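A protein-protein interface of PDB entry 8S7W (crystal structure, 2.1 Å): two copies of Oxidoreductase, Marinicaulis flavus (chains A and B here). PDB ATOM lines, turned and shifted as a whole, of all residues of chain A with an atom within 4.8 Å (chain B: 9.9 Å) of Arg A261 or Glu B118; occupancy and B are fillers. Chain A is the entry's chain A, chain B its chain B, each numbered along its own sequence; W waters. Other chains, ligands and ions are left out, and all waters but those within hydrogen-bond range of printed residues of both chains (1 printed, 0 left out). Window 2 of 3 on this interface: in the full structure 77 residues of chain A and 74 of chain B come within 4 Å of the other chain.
Of the 20 printed residues of chain B, 3 touch a printed residue of chain A. Of the 11 printed residues of chain A, 4 touch a printed residue of chain B. Hydrophobic or aromatic side chains of chain A within 4 Å of the printed part of chain B: Val A265. Among the printed residues, Asp or Glu carboxylates within 4 Å of a Lys or Arg side-chain nitrogen of the other chain: Arg A261 with Glu B118 (3.6 Å).
Water W1 lies within hydrogen-bond range of O of Val A265 (2.6 Å) and OH of Tyr B170 (2.7 Å).
Among the printed residues, merely in contact across the chains: Arg A261 with Phe B119 (3.4 Å), Ile A396 with Phe B119 (3.6 Å), Val A265 with Pro B235 (3.8 Å), Thr A397 with Phe B119 (3.8 Å), Val A265 with Glu B118 (3.9 Å) and Val A265 with Phe B119 (3.96 Å).
No position is printed for both chains. Of the 7 pairs that touch across the chains among the printed residues, none has its exchanged pair printed and touching as well.
NE of Arg A261 is in salt-bridge range of OE1 of Glu B118 (3.6 Å).
No residue of chain B comes within 4 Å of Leu A260. Arg A261 touches two residues of chain B. Pro A262 touches none of the printed residues of chain B. Of the printed residues of chain B, Val A265 touches Glu B118, Phe B119 and Pro B235. Of chain B, only Phe B119 comes within 4 Å of Ile A396. Of the printed residues of chain A, Phe B119 touches Arg A261, Val A265, Ile A396 and Thr A397.
OE1 of Glu A258 lies within salt-bridge range of NH2 of Arg A261 (3.0 Å). The backbone carbonyl oxygen (O) of Ile A396 lies within hydrogen-bond range of the guanidinium group (NH1) of Arg A261 (2.8 Å). The backbone NH (N) of Glu B118 is in hydrogen-bond range of the side-chain amide oxygen (OD1) of Asn B116 (3.3 Å). N of Phe B119 is in hydrogen-bond range of OD1 of Asn B116.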
ATOM      1  N   THR A 257      -0.590  -2.429  -3.062  1.00  0.00           N
ATOM      2  CA  THR A 257      -1.399  -2.225  -1.841  1.00  0.00           C
ATOM      3  C   THR A 257      -2.613  -1.351  -2.171  1.00  0.00           C
ATOM      4  O   THR A 257      -3.690  -1.635  -1.648  1.00  0.00           O
ATOM      5  CB  THR A 257      -0.552  -1.645  -0.708  1.00  0.00           C
ATOM      6  OG1 THR A 257       0.507  -2.566  -0.460  1.00  0.00           O
ATOM      7  CG2 THR A 257      -1.348  -1.442   0.554  1.00  0.00           C
ATOM      8  N   GLU A 258      -2.450  -0.305  -2.996  1.00  0.00           N
ATOM      9  CA  GLU A 258      -3.589   0.540  -3.436  1.00  0.00           C
ATOM     10  C   GLU A 258      -4.653  -0.341  -4.093  1.00  0.00           C
ATOM     11  O   GLU A 258      -5.844  -0.055  -3.925  1.00  0.00           O
ATOM     12  CB  GLU A 258      -3.133   1.582  -4.455  1.00  0.00           C
ATOM     13  CG  GLU A 258      -2.328   2.712  -3.855  1.00  0.00           C
ATOM     14  CD  GLU A 258      -3.149   3.514  -2.862  1.00  0.00           C
ATOM     15  OE1 GLU A 258      -4.142   4.141  -3.326  1.00  0.00           O
ATOM     16  OE2 GLU A 258      -2.823   3.490  -1.640  1.00  0.00           O
ATOM     17  N   ARG A 259      -4.244  -1.318  -4.895  1.00  0.00           N
ATOM     18  CA  ARG A 259      -5.185  -2.136  -5.708  1.00  0.00           C
ATOM     19  C   ARG A 259      -5.830  -3.180  -4.805  1.00  0.00           C
ATOM     20  O   ARG A 259      -7.021  -3.479  -5.003  1.00  0.00           O
ATOM     21  CB  ARG A 259      -4.435  -2.799  -6.858  1.00  0.00           C
ATOM     22  CG  ARG A 259      -3.917  -1.786  -7.872  1.00  0.00           C
ATOM     23  CD  ARG A 259      -2.642  -2.226  -8.564  1.00  0.00           C
ATOM     24  NE  ARG A 259      -2.099  -1.171  -9.410  1.00  0.00           N
ATOM     25  CZ  ARG A 259      -2.208  -1.099 -10.746  1.00  0.00           C
ATOM     26  NH1 ARG A 259      -2.842  -2.024 -11.449  1.00  0.00           N
ATOM     27  NH2 ARG A 259      -1.640  -0.102 -11.388  1.00  0.00           N
ATOM     28  N   LEU A 260      -5.080  -3.678  -3.807  1.00  0.00           N
ATOM     29  CA  LEU A 260      -5.584  -4.682  -2.837  1.00  0.00           C
ATOM     30  C   LEU A 260      -6.711  -4.077  -1.993  1.00  0.00           C
ATOM     31  O   LEU A 260      -7.676  -4.806  -1.674  1.00  0.00           O
ATOM     32  CB  LEU A 260      -4.420  -5.174  -1.972  1.00  0.00           C
ATOM     33  CG  LEU A 260      -3.487  -6.202  -2.614  1.00  0.00           C
ATOM     34  CD1 LEU A 260      -2.293  -6.443  -1.709  1.00  0.00           C
ATOM     35  CD2 LEU A 260      -4.188  -7.521  -2.886  1.00  0.00           C
ATOM     36  N   ARG A 261      -6.652  -2.777  -1.683  1.00  0.00           N
ATOM     37  CA  ARG A 261      -7.575  -2.159  -0.700  1.00  0.00           C
ATOM     38  C   ARG A 261      -9.038  -2.434  -1.046  1.00  0.00           C
ATOM     39  O   ARG A 261      -9.754  -3.029  -0.238  1.00  0.00           O
ATOM     40  CB  ARG A 261      -7.353  -0.654  -0.576  1.00  0.00           C
ATOM     41  CG  ARG A 261      -8.368   0.003   0.342  1.00  0.00           C
ATOM     42  CD  ARG A 261      -8.070   1.462   0.584  1.00  0.00           C
ATOM     43  NE  ARG A 261      -7.930   2.221  -0.642  1.00  0.00           N
ATOM     44  CZ  ARG A 261      -6.793   2.711  -1.125  1.00  0.00           C
ATOM     45  NH1 ARG A 261      -5.621   2.503  -0.538  1.00  0.00           N
ATOM     46  NH2 ARG A 261      -6.838   3.428  -2.231  1.00  0.00           N
ATOM     47  N   PRO A 262      -9.574  -1.997  -2.209  1.00  0.00           N
ATOM     48  CA  PRO A 262     -11.005  -2.179  -2.475  1.00  0.00           C
ATOM     49  C   PRO A 262     -11.376  -3.665  -2.575  1.00  0.00           C
ATOM     50  O   PRO A 262     -12.455  -4.029  -2.258  1.00  0.00           O
ATOM     51  CB  PRO A 262     -11.251  -1.413  -3.790  1.00  0.00           C
ATOM     52  CG  PRO A 262      -9.898  -1.357  -4.457  1.00  0.00           C
ATOM     53  CD  PRO A 262      -8.884  -1.333  -3.322  1.00  0.00           C
ATOM     54  N   LEU A 263     -10.458  -4.503  -3.015  1.00  0.00           N
ATOM     55  CA  LEU A 263     -10.745  -5.941  -3.224  1.00  0.00           C
ATOM     56  C   LEU A 263     -10.919  -6.601  -1.851  1.00  0.00           C
ATOM     57  O   LEU A 263     -11.779  -7.506  -1.716  1.00  0.00           O
ATOM     58  CB  LEU A 263      -9.598  -6.575  -4.008  1.00  0.00           C
ATOM     59  CG  LEU A 263      -9.407  -6.112  -5.458  1.00  0.00           C
ATOM     60  CD1 LEU A 263      -8.099  -6.678  -5.997  1.00  0.00           C
ATOM     61  CD2 LEU A 263     -10.569  -6.554  -6.347  1.00  0.00           C
ATOM     62  N   LYS A 264     -10.178  -6.137  -0.848  1.00  0.00           N
ATOM     63  CA  LYS A 264     -10.247  -6.694   0.532  1.00  0.00           C
ATOM     64  C   LYS A 264     -11.424  -6.091   1.294  1.00  0.00           C
ATOM     65  O   LYS A 264     -12.210  -6.861   1.867  1.00  0.00           O
ATOM     66  CB  LYS A 264      -8.913  -6.499   1.251  1.00  0.00           C
ATOM     67  CG  LYS A 264      -7.864  -7.562   0.950  1.00  0.00           C
ATOM     68  CD  LYS A 264      -8.307  -8.974   1.280  1.00  0.00           C
ATOM     69  CE  LYS A 264      -8.486  -9.282   2.751  1.00  0.00           C
ATOM     70  NZ  LYS A 264      -9.354 -10.475   2.946  1.00  0.00           N
ATOM     71  N   VAL A 265     -11.630  -4.779   1.215  1.00  0.00           N
ATOM     72  CA  VAL A 265     -12.755  -4.119   1.928  1.00  0.00           C
ATOM     73  C   VAL A 265     -14.107  -4.706   1.463  1.00  0.00           C
ATOM     74  O   VAL A 265     -14.993  -4.952   2.350  1.00  0.00           O
ATOM     75  CB  VAL A 265     -12.658  -2.595   1.788  1.00  0.00           C
ATOM     76  CG1 VAL A 265     -13.857  -1.896   2.409  1.00  0.00           C
ATOM     77  CG2 VAL A 265     -11.363  -2.079   2.415  1.00  0.00           C
ATOM     78  N   ILE A 396      -4.585   0.432   4.937  1.00  0.00           N
ATOM     79  CA  ILE A 396      -4.256  -0.215   3.628  1.00  0.00           C
ATOM     80  C   ILE A 396      -4.031   0.899   2.578  1.00  0.00           C
ATOM     81  O   ILE A 396      -4.954   1.194   1.789  1.00  0.00           O
ATOM     82  CB  ILE A 396      -5.327  -1.227   3.163  1.00  0.00           C
ATOM     83  CG1 ILE A 396      -5.861  -2.107   4.296  1.00  0.00           C
ATOM     84  CG2 ILE A 396      -4.782  -2.080   1.996  1.00  0.00           C
ATOM     85  CD1 ILE A 396      -7.150  -2.824   3.934  1.00  0.00           C
ATOM     86  N   THR A 397      -2.856   1.518   2.564  1.00  0.00           N
ATOM     87  CA  THR A 397      -2.451   2.466   1.496  1.00  0.00           C
ATOM     88  C   THR A 397      -1.053   2.055   1.021  1.00  0.00           C
ATOM     89  O   THR A 397      -0.249   1.522   1.858  1.00  0.00           O
ATOM     90  CB  THR A 397      -2.473   3.937   1.953  1.00  0.00           C
ATOM     91  OG1 THR A 397      -1.333   4.179   2.786  1.00  0.00           O
ATOM     92  CG2 THR A 397      -3.743   4.313   2.675  1.00  0.00           C
ATOM     93  N   GLU B 114     -16.546  11.004  11.482  1.00  0.00           N
ATOM     94  CA  GLU B 114     -15.847  10.606  10.225  1.00  0.00           C
ATOM     95  C   GLU B 114     -16.726   9.614   9.470  1.00  0.00           C
ATOM     96  O   GLU B 114     -17.358   8.752  10.132  1.00  0.00           O
ATOM     97  CB  GLU B 114     -14.474   9.953  10.486  1.00  0.00           C
ATOM     98  CG  GLU B 114     -13.587   9.963   9.245  1.00  0.00           C
ATOM     99  CD  GLU B 114     -12.295   9.136   9.190  1.00  0.00           C
ATOM    100  OE1 GLU B 114     -11.823   8.616  10.224  1.00  0.00           O
ATOM    101  OE2 GLU B 114     -11.757   9.006   8.068  1.00  0.00           O
ATOM    102  N   VAL B 115     -16.787   9.751   8.145  1.00  0.00           N
ATOM    103  CA  VAL B 115     -17.270   8.688   7.240  1.00  0.00           C
ATOM    104  C   VAL B 115     -16.150   8.486   6.239  1.00  0.00           C
ATOM    105  O   VAL B 115     -15.780   9.427   5.573  1.00  0.00           O
ATOM    106  CB  VAL B 115     -18.598   9.000   6.533  1.00  0.00           C
ATOM    107  CG1 VAL B 115     -19.063   7.798   5.692  1.00  0.00           C
ATOM    108  CG2 VAL B 115     -19.665   9.392   7.528  1.00  0.00           C
ATOM    109  N   ASN B 116     -15.586   7.296   6.206  1.00  0.00           N
ATOM    110  CA  ASN B 116     -14.416   7.006   5.359  1.00  0.00           C
ATOM    111  C   ASN B 116     -14.878   6.085   4.228  1.00  0.00           C
ATOM    112  O   ASN B 116     -15.314   4.974   4.509  1.00  0.00           O
ATOM    113  CB  ASN B 116     -13.297   6.424   6.216  1.00  0.00           C
ATOM    114  CG  ASN B 116     -12.030   6.342   5.419  1.00  0.00           C
ATOM    115  OD1 ASN B 116     -12.008   5.706   4.365  1.00  0.00           O
ATOM    116  ND2 ASN B 116     -10.993   7.016   5.888  1.00  0.00           N
ATOM    117  N   GLU B 117     -14.813   6.535   2.993  1.00  0.00           N
ATOM    118  CA  GLU B 117     -15.312   5.750   1.840  1.00  0.00           C
ATOM    119  C   GLU B 117     -14.333   4.634   1.470  1.00  0.00           C
ATOM    120  O   GLU B 117     -14.808   3.538   1.223  1.00  0.00           O
ATOM    121  CB  GLU B 117     -15.571   6.661   0.642  1.00  0.00           C
ATOM    122  CG  GLU B 117     -16.239   5.923  -0.502  1.00  0.00           C
ATOM    123  CD  GLU B 117     -16.466   6.849  -1.685  1.00  0.00           C
ATOM    124  OE1 GLU B 117     -15.492   7.477  -2.132  1.00  0.00           O
ATOM    125  OE2 GLU B 117     -17.612   7.020  -2.068  1.00  0.00           O
ATOM    126  N   GLU B 118     -13.034   4.905   1.376  1.00  0.00           N
ATOM    127  CA  GLU B 118     -12.035   3.919   0.877  1.00  0.00           C
ATOM    128  C   GLU B 118     -11.868   2.779   1.898  1.00  0.00           C
ATOM    129  O   GLU B 118     -11.562   1.668   1.458  1.00  0.00           O
ATOM    130  CB  GLU B 118     -10.690   4.585   0.545  1.00  0.00           C
ATOM    131  CG  GLU B 118      -9.988   5.183   1.752  1.00  0.00           C
ATOM    132  CD  GLU B 118      -8.727   5.983   1.477  1.00  0.00           C
ATOM    133  OE1 GLU B 118      -8.011   5.641   0.516  1.00  0.00           O
ATOM    134  OE2 GLU B 118      -8.453   6.944   2.256  1.00  0.00           O
ATOM    135  N   PHE B 119     -12.089   3.014   3.198  1.00  0.00           N
ATOM    136  CA  PHE B 119     -11.959   1.953   4.231  1.00  0.00           C
ATOM    137  C   PHE B 119     -13.331   1.482   4.696  1.00  0.00           C
ATOM    138  O   PHE B 119     -13.372   0.544   5.492  1.00  0.00           O
ATOM    139  CB  PHE B 119     -11.092   2.419   5.401  1.00  0.00           C
ATOM    140  CG  PHE B 119      -9.692   2.807   5.001  1.00  0.00           C
ATOM    141  CD1 PHE B 119      -8.918   1.954   4.245  1.00  0.00           C
ATOM    142  CD2 PHE B 119      -9.136   4.003   5.423  1.00  0.00           C
ATOM    143  CE1 PHE B 119      -7.623   2.300   3.894  1.00  0.00           C
ATOM    144  CE2 PHE B 119      -7.837   4.341   5.081  1.00  0.00           C
ATOM    145  CZ  PHE B 119      -7.100   3.506   4.291  1.00  0.00           C
ATOM    146  N   GLY B 120     -14.410   2.098   4.211  1.00  0.00           N
ATOM    147  CA  GLY B 120     -15.795   1.709   4.554  1.00  0.00           C
ATOM    148  C   GLY B 120     -16.036   1.675   6.051  1.00  0.00           C
ATOM    149  O   GLY B 120     -16.237   0.574   6.608  1.00  0.00           O
ATOM    150  N   TYR B 121     -16.079   2.841   6.701  1.00  0.00           N
ATOM    151  CA  TYR B 121     -16.424   2.915   8.135  1.00  0.00           C
ATOM    152  C   TYR B 121     -16.998   4.291   8.477  1.00  0.00           C
ATOM    153  O   TYR B 121     -16.819   5.250   7.706  1.00  0.00           O
ATOM    154  CB  TYR B 121     -15.198   2.556   8.993  1.00  0.00           C
ATOM    155  CG  TYR B 121     -14.105   3.589   9.112  1.00  0.00           C
ATOM    156  CD1 TYR B 121     -14.251   4.726   9.908  1.00  0.00           C
ATOM    157  CD2 TYR B 121     -12.877   3.393   8.506  1.00  0.00           C
ATOM    158  CE1 TYR B 121     -13.223   5.646  10.048  1.00  0.00           C
ATOM    159  CE2 TYR B 121     -11.830   4.287   8.667  1.00  0.00           C
ATOM    160  CZ  TYR B 121     -12.004   5.420   9.435  1.00  0.00           C
ATOM    161  OH  TYR B 121     -10.971   6.313   9.599  1.00  0.00           O
ATOM    162  N   ALA B 122     -17.628   4.376   9.640  1.00  0.00           N
ATOM    163  CA  ALA B 122     -18.054   5.654  10.245  1.00  0.00           C
ATOM    164  C   ALA B 122     -17.670   5.663  11.728  1.00  0.00           C
ATOM    165  O   ALA B 122     -17.650   4.577  12.385  1.00  0.00           O
ATOM    166  CB  ALA B 122     -19.532   5.872  10.067  1.00  0.00           C
ATOM    167  N   LEU B 142     -21.239   9.403  -1.164  1.00  0.00           N
ATOM    168  CA  LEU B 142     -20.277   8.309  -0.812  1.00  0.00           C
ATOM    169  C   LEU B 142     -20.900   6.959  -1.211  1.00  0.00           C
ATOM    170  O   LEU B 142     -22.081   6.757  -0.937  1.00  0.00           O
ATOM    171  CB  LEU B 142     -19.926   8.395   0.676  1.00  0.00           C
ATOM    172  CG  LEU B 142     -19.343   9.749   1.086  1.00  0.00           C
ATOM    173  CD1 LEU B 142     -19.189   9.866   2.590  1.00  0.00           C
ATOM    174  CD2 LEU B 142     -18.017  10.013   0.383  1.00  0.00           C
ATOM    175  N   LYS B 143     -20.147   6.081  -1.872  1.00  0.00           N
ATOM    176  CA  LYS B 143     -20.635   4.750  -2.314  1.00  0.00           C
ATOM    177  C   LYS B 143     -20.591   3.762  -1.138  1.00  0.00           C
ATOM    178  O   LYS B 143     -19.906   2.706  -1.238  1.00  0.00           O
ATOM    179  CB  LYS B 143     -19.824   4.315  -3.534  1.00  0.00           C
ATOM    180  CG  LYS B 143     -19.922   5.303  -4.698  1.00  0.00           C
ATOM    181  CD  LYS B 143     -19.089   4.933  -5.929  1.00  0.00           C
ATOM    182  CE  LYS B 143     -17.584   4.909  -5.710  1.00  0.00           C
ATOM    183  NZ  LYS B 143     -17.048   6.216  -5.241  1.00  0.00           N
ATOM    184  N   LEU B 144     -21.345   4.059  -0.080  1.00  0.00           N
ATOM    185  CA  LEU B 144     -21.457   3.164   1.100  1.00  0.00           C
ATOM    186  C   LEU B 144     -22.926   2.913   1.421  1.00  0.00           C
ATOM    187  O   LEU B 144     -23.733   3.864   1.284  1.00  0.00           O
ATOM    188  CB  LEU B 144     -20.762   3.817   2.299  1.00  0.00           C
ATOM    189  CG  LEU B 144     -19.282   4.151   2.113  1.00  0.00           C
ATOM    190  CD1 LEU B 144     -18.854   5.092   3.209  1.00  0.00           C
ATOM    191  CD2 LEU B 144     -18.405   2.899   2.080  1.00  0.00           C
ATOM    192  N   TYR B 170     -24.289  -6.818   6.615  1.00  0.00           N
ATOM    193  CA  TYR B 170     -23.760  -6.166   7.839  1.00  0.00           C
ATOM    194  C   TYR B 170     -24.823  -6.133   8.949  1.00  0.00           C
ATOM    195  O   TYR B 170     -24.798  -5.195   9.785  1.00  0.00           O
ATOM    196  CB  TYR B 170     -23.248  -4.759   7.528  1.00  0.00           C
ATOM    197  CG  TYR B 170     -21.892  -4.682   6.862  1.00  0.00           C
ATOM    198  CD1 TYR B 170     -21.577  -5.451   5.737  1.00  0.00           C
ATOM    199  CD2 TYR B 170     -20.931  -3.804   7.344  1.00  0.00           C
ATOM    200  CE1 TYR B 170     -20.323  -5.369   5.139  1.00  0.00           C
ATOM    201  CE2 TYR B 170     -19.682  -3.712   6.744  1.00  0.00           C
ATOM    202  CZ  TYR B 170     -19.378  -4.473   5.627  1.00  0.00           C
ATOM    203  OH  TYR B 170     -18.149  -4.330   5.047  1.00  0.00           O
ATOM    204  N   ASN B 201      -4.149   5.801  12.934  1.00  0.00           N
ATOM    205  CA  ASN B 201      -5.255   6.013  11.957  1.00  0.00           C
ATOM    206  C   ASN B 201      -5.973   4.667  11.743  1.00  0.00           C
ATOM    207  O   ASN B 201      -6.399   4.397  10.611  1.00  0.00           O
ATOM    208  CB  ASN B 201      -4.718   6.632  10.658  1.00  0.00           C
ATOM    209  CG  ASN B 201      -4.097   7.987  10.899  1.00  0.00           C
ATOM    210  OD1 ASN B 201      -2.889   8.133  11.077  1.00  0.00           O
ATOM    211  ND2 ASN B 201      -4.920   8.994  10.925  1.00  0.00           N
ATOM    212  N   GLN B 204     -10.732   2.383  13.541  1.00  0.00           N
ATOM    213  CA  GLN B 204     -11.893   1.744  12.854  1.00  0.00           C
ATOM    214  C   GLN B 204     -11.424   0.696  11.839  1.00  0.00           C
ATOM    215  O   GLN B 204     -12.252   0.269  11.019  1.00  0.00           O
ATOM    216  CB  GLN B 204     -12.774   2.813  12.190  1.00  0.00           C
ATOM    217  CG  GLN B 204     -13.766   3.426  13.171  1.00  0.00           C
ATOM    218  CD  GLN B 204     -13.115   4.211  14.295  1.00  0.00           C
ATOM    219  OE1 GLN B 204     -12.577   5.285  14.105  1.00  0.00           O
ATOM    220  NE2 GLN B 204     -13.174   3.701  15.505  1.00  0.00           N
ATOM    221  N   LEU B 205     -10.171   0.282  11.866  1.00  0.00           N
ATOM    222  CA  LEU B 205      -9.648  -0.708  10.875  1.00  0.00           C
ATOM    223  C   LEU B 205      -9.357  -2.071  11.518  1.00  0.00           C
ATOM    224  O   LEU B 205      -9.258  -3.066  10.755  1.00  0.00           O
ATOM    225  CB  LEU B 205      -8.388  -0.176  10.186  1.00  0.00           C
ATOM    226  CG  LEU B 205      -8.526   1.187   9.516  1.00  0.00           C
ATOM    227  CD1 LEU B 205      -7.268   1.538   8.756  1.00  0.00           C
ATOM    228  CD2 LEU B 205      -9.736   1.212   8.594  1.00  0.00           C
ATOM    229  N   LEU B 233     -18.903  -0.156   7.430  1.00  0.00           N
ATOM    230  CA  LEU B 233     -19.975   0.149   6.444  1.00  0.00           C
ATOM    231  C   LEU B 233     -19.680  -0.631   5.170  1.00  0.00           C
ATOM    232  O   LEU B 233     -18.526  -0.624   4.728  1.00  0.00           O
ATOM    233  CB  LEU B 233     -20.012   1.651   6.130  1.00  0.00           C
ATOM    234  CG  LEU B 233     -20.428   2.583   7.276  1.00  0.00           C
ATOM    235  CD1 LEU B 233     -20.467   4.019   6.791  1.00  0.00           C
ATOM    236  CD2 LEU B 233     -21.776   2.183   7.873  1.00  0.00           C
ATOM    237  N   MET B 234     -20.696  -1.248   4.598  1.00  0.00           N
ATOM    238  CA  MET B 234     -20.561  -2.052   3.366  1.00  0.00           C
ATOM    239  C   MET B 234     -20.344  -1.132   2.158  1.00  0.00           C
ATOM    240  O   MET B 234     -21.097  -0.202   1.912  1.00  0.00           O
ATOM    241  CB  MET B 234     -21.818  -2.891   3.147  1.00  0.00           C
ATOM    242  CG  MET B 234     -21.634  -3.915   2.043  1.00  0.00           C
ATOM    243  SD  MET B 234     -23.030  -5.059   1.926  1.00  0.00           S
ATOM    244  CE  MET B 234     -24.327  -3.883   1.581  1.00  0.00           C
ATOM    245  N   PRO B 235     -19.293  -1.336   1.350  1.00  0.00           N
ATOM    246  CA  PRO B 235     -19.209  -0.682   0.047  1.00  0.00           C
ATOM    247  C   PRO B 235     -20.453  -0.985  -0.801  1.00  0.00           C
ATOM    248  O   PRO B 235     -20.921  -2.115  -0.795  1.00  0.00           O
ATOM    249  CB  PRO B 235     -17.951  -1.283  -0.592  1.00  0.00           C
ATOM    250  CG  PRO B 235     -17.142  -1.725   0.598  1.00  0.00           C
ATOM    251  CD  PRO B 235     -18.151  -2.192   1.621  1.00  0.00           C
ATOM    252  N   GLU B 236     -20.994   0.030  -1.455  1.00  0.00           N
ATOM    253  CA  GLU B 236     -22.075  -0.170  -2.443  1.00  0.00           C
ATOM    254  C   GLU B 236     -21.673  -1.331  -3.341  1.00  0.00           C
ATOM    255  O   GLU B 236     -20.632  -1.293  -3.971  1.00  0.00           O
ATOM    256  CB  GLU B 236     -22.278   1.091  -3.285  1.00  0.00           C
ATOM    257  CG  GLU B 236     -23.454   0.988  -4.214  1.00  0.00           C
ATOM    258  CD  GLU B 236     -23.675   2.202  -5.102  1.00  0.00           C
ATOM    259  OE1 GLU B 236     -22.738   3.015  -5.245  1.00  0.00           O
ATOM    260  OE2 GLU B 236     -24.784   2.307  -5.664  1.00  0.00           O
HETATM  261  O   HOH W   1     -17.476  -5.630   2.806  1.00  0.00           O
